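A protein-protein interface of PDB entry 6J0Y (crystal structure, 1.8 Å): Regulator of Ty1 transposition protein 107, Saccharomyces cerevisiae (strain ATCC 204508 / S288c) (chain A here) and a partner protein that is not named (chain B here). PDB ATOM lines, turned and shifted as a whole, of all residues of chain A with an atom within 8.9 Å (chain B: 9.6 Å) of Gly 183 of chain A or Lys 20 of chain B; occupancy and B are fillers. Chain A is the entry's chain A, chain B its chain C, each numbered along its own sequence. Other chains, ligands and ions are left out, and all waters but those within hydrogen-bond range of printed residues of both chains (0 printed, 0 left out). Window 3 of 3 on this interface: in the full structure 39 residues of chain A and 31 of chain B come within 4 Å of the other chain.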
ATOM      1  N   LYS A 179      27.731   9.797   3.727  1.00  0.00           N
ATOM      2  CA  LYS A 179      26.357   9.591   3.298  1.00  0.00           C
ATOM      3  C   LYS A 179      25.696   8.369   3.936  1.00  0.00           C
ATOM      4  O   LYS A 179      24.555   8.051   3.581  1.00  0.00           O
ATOM      5  CB  LYS A 179      26.299   9.478   1.770  1.00  0.00           C
ATOM      6  CG  LYS A 179      26.455  10.825   1.065  1.00  0.00           C
ATOM      7  CD  LYS A 179      26.274  10.698  -0.433  1.00  0.00           C
ATOM      8  CE  LYS A 179      25.910  12.037  -1.068  1.00  0.00           C
ATOM      9  NZ  LYS A 179      26.945  13.076  -0.825  1.00  0.00           N
ATOM     10  N   LEU A 180      26.371   7.681   4.862  1.00  0.00           N
ATOM     11  CA  LEU A 180      25.789   6.529   5.561  1.00  0.00           C
ATOM     12  C   LEU A 180      24.802   7.046   6.602  1.00  0.00           C
ATOM     13  O   LEU A 180      25.080   7.117   7.804  1.00  0.00           O
ATOM     14  CB  LEU A 180      26.877   5.667   6.192  1.00  0.00           C
ATOM     15  CG  LEU A 180      27.792   4.917   5.222  1.00  0.00           C
ATOM     16  CD1 LEU A 180      28.921   4.229   5.971  1.00  0.00           C
ATOM     17  CD2 LEU A 180      26.989   3.892   4.397  1.00  0.00           C
ATOM     18  N   THR A 181      23.616   7.413   6.124  1.00  0.00           N
ATOM     19  CA  THR A 181      22.597   8.034   6.953  1.00  0.00           C
ATOM     20  C   THR A 181      21.293   7.257   6.844  1.00  0.00           C
ATOM     21  O   THR A 181      21.063   6.523   5.877  1.00  0.00           O
ATOM     22  CB  THR A 181      22.368   9.504   6.556  1.00  0.00           C
ATOM     23  OG1 THR A 181      22.010   9.582   5.168  1.00  0.00           O
ATOM     24  CG2 THR A 181      23.631  10.336   6.801  1.00  0.00           C
ATOM     25  N   PHE A 182      20.434   7.439   7.848  1.00  0.00           N
ATOM     26  CA  PHE A 182      19.182   6.702   7.957  1.00  0.00           C
ATOM     27  C   PHE A 182      18.028   7.665   8.194  1.00  0.00           C
ATOM     28  O   PHE A 182      18.126   8.574   9.025  1.00  0.00           O
ATOM     29  CB  PHE A 182      19.249   5.672   9.092  1.00  0.00           C
ATOM     30  CG  PHE A 182      20.426   4.752   8.991  1.00  0.00           C
ATOM     31  CD1 PHE A 182      21.658   5.122   9.513  1.00  0.00           C
ATOM     32  CD2 PHE A 182      20.309   3.527   8.362  1.00  0.00           C
ATOM     33  CE1 PHE A 182      22.750   4.285   9.410  1.00  0.00           C
ATOM     34  CE2 PHE A 182      21.396   2.684   8.260  1.00  0.00           C
ATOM     35  CZ  PHE A 182      22.620   3.064   8.786  1.00  0.00           C
ATOM     36  N   GLY A 183      16.935   7.459   7.467  1.00  0.00           N
ATOM     37  CA  GLY A 183      15.761   8.301   7.611  1.00  0.00           C
ATOM     38  C   GLY A 183      14.543   7.757   6.893  1.00  0.00           C
ATOM     39  O   GLY A 183      14.384   6.543   6.748  1.00  0.00           O
ATOM     40  N   GLU A 195      17.361  12.227   9.073  1.00  0.00           N
ATOM     41  CA  GLU A 195      18.609  11.655   8.573  1.00  0.00           C
ATOM     42  C   GLU A 195      19.660  11.531   9.674  1.00  0.00           C
ATOM     43  O   GLU A 195      20.487  12.425   9.858  1.00  0.00           O
ATOM     44  CB  GLU A 195      19.161  12.497   7.422  1.00  0.00           C
ATOM     45  CG  GLU A 195      18.247  12.566   6.211  1.00  0.00           C
ATOM     46  CD  GLU A 195      18.804  13.450   5.112  1.00  0.00           C
ATOM     47  OE1 GLU A 195      20.004  13.317   4.794  1.00  0.00           O
ATOM     48  OE2 GLU A 195      18.045  14.286   4.576  1.00  0.00           O
ATOM     49  N   LYS A 196      19.626  10.408  10.403  1.00  0.00           N
ATOM     50  CA  LYS A 196      20.577  10.164  11.485  1.00  0.00           C
ATOM     51  C   LYS A 196      21.833   9.496  10.939  1.00  0.00           C
ATOM     52  O   LYS A 196      21.730   8.538  10.164  1.00  0.00           O
ATOM     53  CB  LYS A 196      19.961   9.286  12.564  1.00  0.00           C
ATOM     54  CG  LYS A 196      18.759   9.902  13.254  1.00  0.00           C
ATOM     55  CD  LYS A 196      18.338   9.088  14.469  1.00  0.00           C
ATOM     56  CE  LYS A 196      17.125   9.711  15.157  1.00  0.00           C
ATOM     57  NZ  LYS A 196      16.751   8.982  16.403  1.00  0.00           N
ATOM     58  N   PRO A 197      23.021   9.960  11.316  1.00  0.00           N
ATOM     59  CA  PRO A 197      24.248   9.309  10.848  1.00  0.00           C
ATOM     60  C   PRO A 197      24.500   7.998  11.574  1.00  0.00           C
ATOM     61  O   PRO A 197      24.045   7.778  12.699  1.00  0.00           O
ATOM     62  CB  PRO A 197      25.339  10.340  11.170  1.00  0.00           C
ATOM     63  CG  PRO A 197      24.797  11.105  12.324  1.00  0.00           C
ATOM     64  CD  PRO A 197      23.301  11.149  12.143  1.00  0.00           C
ATOM     65  N   LEU B  13      25.888  -3.248   9.348  1.00  0.00           N
ATOM     66  CA  LEU B  13      24.667  -2.534   9.693  1.00  0.00           C
ATOM     67  C   LEU B  13      23.713  -3.488  10.397  1.00  0.00           C
ATOM     68  O   LEU B  13      23.657  -4.668  10.060  1.00  0.00           O
ATOM     69  CB  LEU B  13      23.969  -2.024   8.416  1.00  0.00           C
ATOM     70  CG  LEU B  13      23.827  -0.544   8.120  1.00  0.00           C
ATOM     71  CD1 LEU B  13      25.089   0.179   8.522  1.00  0.00           C
ATOM     72  CD2 LEU B  13      23.534  -0.358   6.637  1.00  0.00           C
ATOM     73  N   LEU B  14      22.925  -2.970  11.335  1.00  0.00           N
ATOM     74  CA  LEU B  14      21.794  -3.752  11.833  1.00  0.00           C
ATOM     75  C   LEU B  14      20.843  -4.071  10.682  1.00  0.00           C
ATOM     76  O   LEU B  14      20.557  -3.217   9.840  1.00  0.00           O
ATOM     77  CB  LEU B  14      21.053  -2.991  12.936  1.00  0.00           C
ATOM     78  CG  LEU B  14      21.711  -3.013  14.315  1.00  0.00           C
ATOM     79  CD1 LEU B  14      20.947  -2.138  15.310  1.00  0.00           C
ATOM     80  CD2 LEU B  14      21.802  -4.445  14.828  1.00  0.00           C
ATOM     81  N   GLN B  15      20.388  -5.330  10.625  1.00  0.00           N
ATOM     82  CA  GLN B  15      19.468  -5.746   9.569  1.00  0.00           C
ATOM     83  C   GLN B  15      18.256  -4.823   9.490  1.00  0.00           C
ATOM     84  O   GLN B  15      17.814  -4.457   8.394  1.00  0.00           O
ATOM     85  CB  GLN B  15      19.034  -7.199   9.802  1.00  0.00           C
ATOM     86  CG  GLN B  15      18.149  -7.778   8.710  1.00  0.00           C
ATOM     87  CD  GLN B  15      16.675  -7.684   9.047  1.00  0.00           C
ATOM     88  OE1 GLN B  15      16.259  -7.996  10.165  1.00  0.00           O
ATOM     89  NE2 GLN B  15      15.872  -7.253   8.077  1.00  0.00           N
ATOM     90  N   GLU B  16      17.721  -4.428  10.650  1.00  0.00           N
ATOM     91  CA  GLU B  16      16.614  -3.473  10.710  1.00  0.00           C
ATOM     92  C   GLU B  16      16.931  -2.171   9.990  1.00  0.00           C
ATOM     93  O   GLU B  16      16.019  -1.509   9.479  1.00  0.00           O
ATOM     94  CB  GLU B  16      16.273  -3.153  12.167  1.00  0.00           C
ATOM     95  CG  GLU B  16      15.612  -4.264  12.947  1.00  0.00           C
ATOM     96  CD  GLU B  16      15.456  -3.909  14.415  1.00  0.00           C
ATOM     97  OE1 GLU B  16      16.382  -3.277  14.976  1.00  0.00           O
ATOM     98  OE2 GLU B  16      14.408  -4.249  15.004  1.00  0.00           O
ATOM     99  N   SER B  17      18.204  -1.777   9.959  1.00  0.00           N
ATOM    100  CA  SER B  17      18.590  -0.464   9.456  1.00  0.00           C
ATOM    101  C   SER B  17      18.657  -0.399   7.941  1.00  0.00           C
ATOM    102  O   SER B  17      18.663   0.705   7.391  1.00  0.00           O
ATOM    103  CB  SER B  17      19.956  -0.057  10.019  1.00  0.00           C
ATOM    104  OG  SER B  17      19.956  -0.106  11.433  1.00  0.00           O
ATOM    105  N   VAL B  18      18.715  -1.549   7.264  1.00  0.00           N
ATOM    106  CA  VAL B  18      18.991  -1.561   5.831  1.00  0.00           C
ATOM    107  C   VAL B  18      17.888  -0.853   5.063  1.00  0.00           C
ATOM    108  O   VAL B  18      18.153  -0.048   4.161  1.00  0.00           O
ATOM    109  CB  VAL B  18      19.175  -3.001   5.334  1.00  0.00           C
ATOM    110  CG1 VAL B  18      19.382  -3.022   3.833  1.00  0.00           C
ATOM    111  CG2 VAL B  18      20.336  -3.597   6.026  1.00  0.00           C
ATOM    112  N   VAL B  19      16.632  -1.152   5.405  1.00  0.00           N
ATOM    113  CA  VAL B  19      15.503  -0.554   4.705  1.00  0.00           C
ATOM    114  C   VAL B  19      15.482   0.961   4.882  1.00  0.00           C
ATOM    115  O   VAL B  19      14.890   1.669   4.063  1.00  0.00           O
ATOM    116  CB  VAL B  19      14.188  -1.216   5.185  1.00  0.00           C
ATOM    117  CG1 VAL B  19      13.831  -0.774   6.604  1.00  0.00           C
ATOM    118  CG2 VAL B  19      13.049  -0.939   4.211  1.00  0.00           C
ATOM    119  N   LYS B  20      16.141   1.479   5.921  1.00  0.00           N
ATOM    120  CA  LYS B  20      16.192   2.909   6.195  1.00  0.00           C
ATOM    121  C   LYS B  20      17.462   3.576   5.678  1.00  0.00           C
ATOM    122  O   LYS B  20      17.614   4.791   5.829  1.00  0.00           O
ATOM    123  CB  LYS B  20      16.070   3.161   7.700  1.00  0.00           C
ATOM    124  CG  LYS B  20      14.874   2.494   8.354  1.00  0.00           C
ATOM    125  CD  LYS B  20      14.986   2.575   9.869  1.00  0.00           C
ATOM    126  CE  LYS B  20      13.868   1.821  10.566  1.00  0.00           C
ATOM    127  NZ  LYS B  20      14.018   1.899  12.045  1.00  0.00           N
ATOM    128  N   LEU B  21      18.378   2.818   5.083  1.00  0.00           N
ATOM    129  CA  LEU B  21      19.633   3.393   4.626  1.00  0.00           C
ATOM    130  C   LEU B  21      19.339   4.380   3.503  1.00  0.00           C
ATOM    131  O   LEU B  21      18.378   4.208   2.747  1.00  0.00           O
ATOM    132  CB  LEU B  21      20.607   2.283   4.235  1.00  0.00           C
ATOM    133  CG  LEU B  21      21.967   2.721   3.699  1.00  0.00           C
ATOM    134  CD1 LEU B  21      22.794   3.348   4.814  1.00  0.00           C
ATOM    135  CD2 LEU B  21      22.688   1.546   3.089  1.00  0.00           C
ATOM    136  N   ASN B  22      20.181   5.428   3.407  1.00  0.00           N
ATOM    137  CA  ASN B  22      20.151   6.470   2.379  1.00  0.00           C
ATOM    138  C   ASN B  22      19.874   5.786   1.045  1.00  0.00           C
ATOM    139  O   ASN B  22      20.679   4.966   0.589  1.00  0.00           O
ATOM    140  CB  ASN B  22      21.490   7.211   2.385  1.00  0.00           C
ATOM    141  CG  ASN B  22      21.540   8.366   1.400  1.00  0.00           C
ATOM    142  OD1 ASN B  22      20.670   8.516   0.539  1.00  0.00           O
ATOM    143  ND2 ASN B  22      22.578   9.186   1.515  1.00  0.00           N
ATOM    144  N   PRO B  23      18.743   6.087   0.398  1.00  0.00           N
ATOM    145  CA  PRO B  23      18.412   5.408  -0.864  1.00  0.00           C
ATOM    146  C   PRO B  23      19.291   5.883  -2.010  1.00  0.00           C
ATOM    147  O   PRO B  23      19.302   5.234  -3.062  1.00  0.00           O
ATOM    148  CB  PRO B  23      16.940   5.778  -1.103  1.00  0.00           C
ATOM    149  CG  PRO B  23      16.704   6.982  -0.266  1.00  0.00           C
ATOM    150  CD  PRO B  23      17.574   6.817   0.945  1.00  0.00           C
ATOM    151  N   LYS B  24      20.028   6.980  -1.847  1.00  0.00           N
ATOM    152  CA  LYS B  24      20.893   7.470  -2.912  1.00  0.00           C
ATOM    153  C   LYS B  24      22.216   6.719  -2.998  1.00  0.00           C
ATOM    154  O   LYS B  24      22.928   6.867  -3.995  1.00  0.00           O
ATOM    155  CB  LYS B  24      21.130   8.973  -2.727  1.00  0.00           C
ATOM    156  CG  LYS B  24      19.899   9.804  -3.076  1.00  0.00           C
ATOM    157  CD  LYS B  24      19.967  11.236  -2.567  1.00  0.00           C
ATOM    158  CE  LYS B  24      18.701  11.997  -2.962  1.00  0.00           C
ATOM    159  NZ  LYS B  24      18.595  13.348  -2.335  1.00  0.00           N
ATOM    160  N   LEU B  25      22.555   5.916  -1.993  1.00  0.00           N
ATOM    161  CA  LEU B  25      23.708   5.031  -2.080  1.00  0.00           C
ATOM    162  C   LEU B  25      23.363   3.802  -2.917  1.00  0.00           C
ATOM    163  O   LEU B  25      22.273   3.237  -2.794  1.00  0.00           O
ATOM    164  CB  LEU B  25      24.157   4.601  -0.680  1.00  0.00           C
ATOM    165  CG  LEU B  25      24.677   5.697   0.261  1.00  0.00           C
ATOM    166  CD1 LEU B  25      24.878   5.157   1.677  1.00  0.00           C
ATOM    167  CD2 LEU B  25      25.976   6.290  -0.256  1.00  0.00           C
ATOM    168  N   LYS B  27      23.793   0.023  -3.570  1.00  0.00           N
ATOM    169  CA  LYS B  27      24.179  -1.220  -2.913  1.00  0.00           C
ATOM    170  C   LYS B  27      24.524  -2.260  -3.971  1.00  0.00           C
ATOM    171  O   LYS B  27      23.661  -2.645  -4.766  1.00  0.00           O
ATOM    172  CB  LYS B  27      23.050  -1.744  -2.026  1.00  0.00           C
ATOM    173  CG  LYS B  27      22.600  -0.802  -0.925  1.00  0.00           C
ATOM    174  CD  LYS B  27      21.195  -1.172  -0.456  1.00  0.00           C
ATOM    175  CE  LYS B  27      20.804  -0.424   0.810  1.00  0.00           C
ATOM    176  NZ  LYS B  27      19.344  -0.518   1.108  1.00  0.00           N
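Among the printed residues, merely in contact across the chains: Lys 179 of chain A with Leu 25 of chain B (3.5 Å), Leu 180 of chain A with Leu 25 of chain B (3.7 Å), Thr 181 of chain A with Lys 20 of chain B (3.9 Å), Thr 181 of chain A with Leu 21 of chain B (3.6 Å), Phe 182 of chain A with Leu 13 of chain B (3.8 Å), Phe 182 of chain A with Ser 17 of chain B (3.4 Å), Phe 182 of chain A with Lys 20 of chain B (3.3 Å) and Phe 182 of chain A with Leu 21 of chain B (3.8 Å).
The backbone carbonyl oxygen (O) of Lys 179 of chain A sits at hydrogen-bond distance from the side-chain hydroxyl (OG1) of Thr 181 of chain A, at 3.4 Å. The backbone carbonyl oxygen of Phe 182 of chain A is in hydrogen-bond range of the backbone NH of Lys 196 of chain A. OD1 of Asn 22 of chain B is in hydrogen-bond range of N of Lys 24 of chain B (2.9 Å).
Of the 8 printed residues of chain A, 5 touch a printed residue of chain B. Of the 14 printed residues of chain B, 6 touch a printed residue of chain A. Among the printed residues, 11 pairs touch across the chains. Among the printed residues, no Asp or Glu carboxylate lies within 4 Å of a Lys or Arg side-chain nitrogen of the other chain.
The backbone carbonyl oxygen (O) of Lys 179 of chain A is in hydrogen-bond range of the side-chain amide nitrogen (ND2) of Asn 22 of chain B (3.1 Å). The backbone carbonyl oxygen (O) of Thr 181 of chain A is in hydrogen-bond range of the backbone NH (N) of Asn 22 of chain B, 2.8 Å away. The backbone carbonyl oxygen of Lys 20 of chain B sits at hydrogen-bond distance from the backbone NH of Gly 183 of chain A (3.2 Å).
Lys 20 of chain B touches three residues of chain A. No residue of chain A comes within 4 Å of Val 19 of chain B. Of the printed residues of chain B, Leu 180 of chain A touches Leu 25 (3.7 Å). Of the printed residues of chain B, Phe 182 of chain A touches Leu 13 (3.8 Å), Ser 17 (3.4 Å), Lys 20 (3.3 Å) and Leu 21 (3.8 Å). Lys 196 of chain A touches none of the printed residues of chain B. Lys 27 of chain B touches none of the printed residues of chain A. The nearest residue of chain A that does not touch Lys 20 of chain B is Lys 196 of chain A (7.1 Å). The nearest printed residue of chain A that does not touch Asn 22 of chain B is Phe 182 of chain A (4.8 Å).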
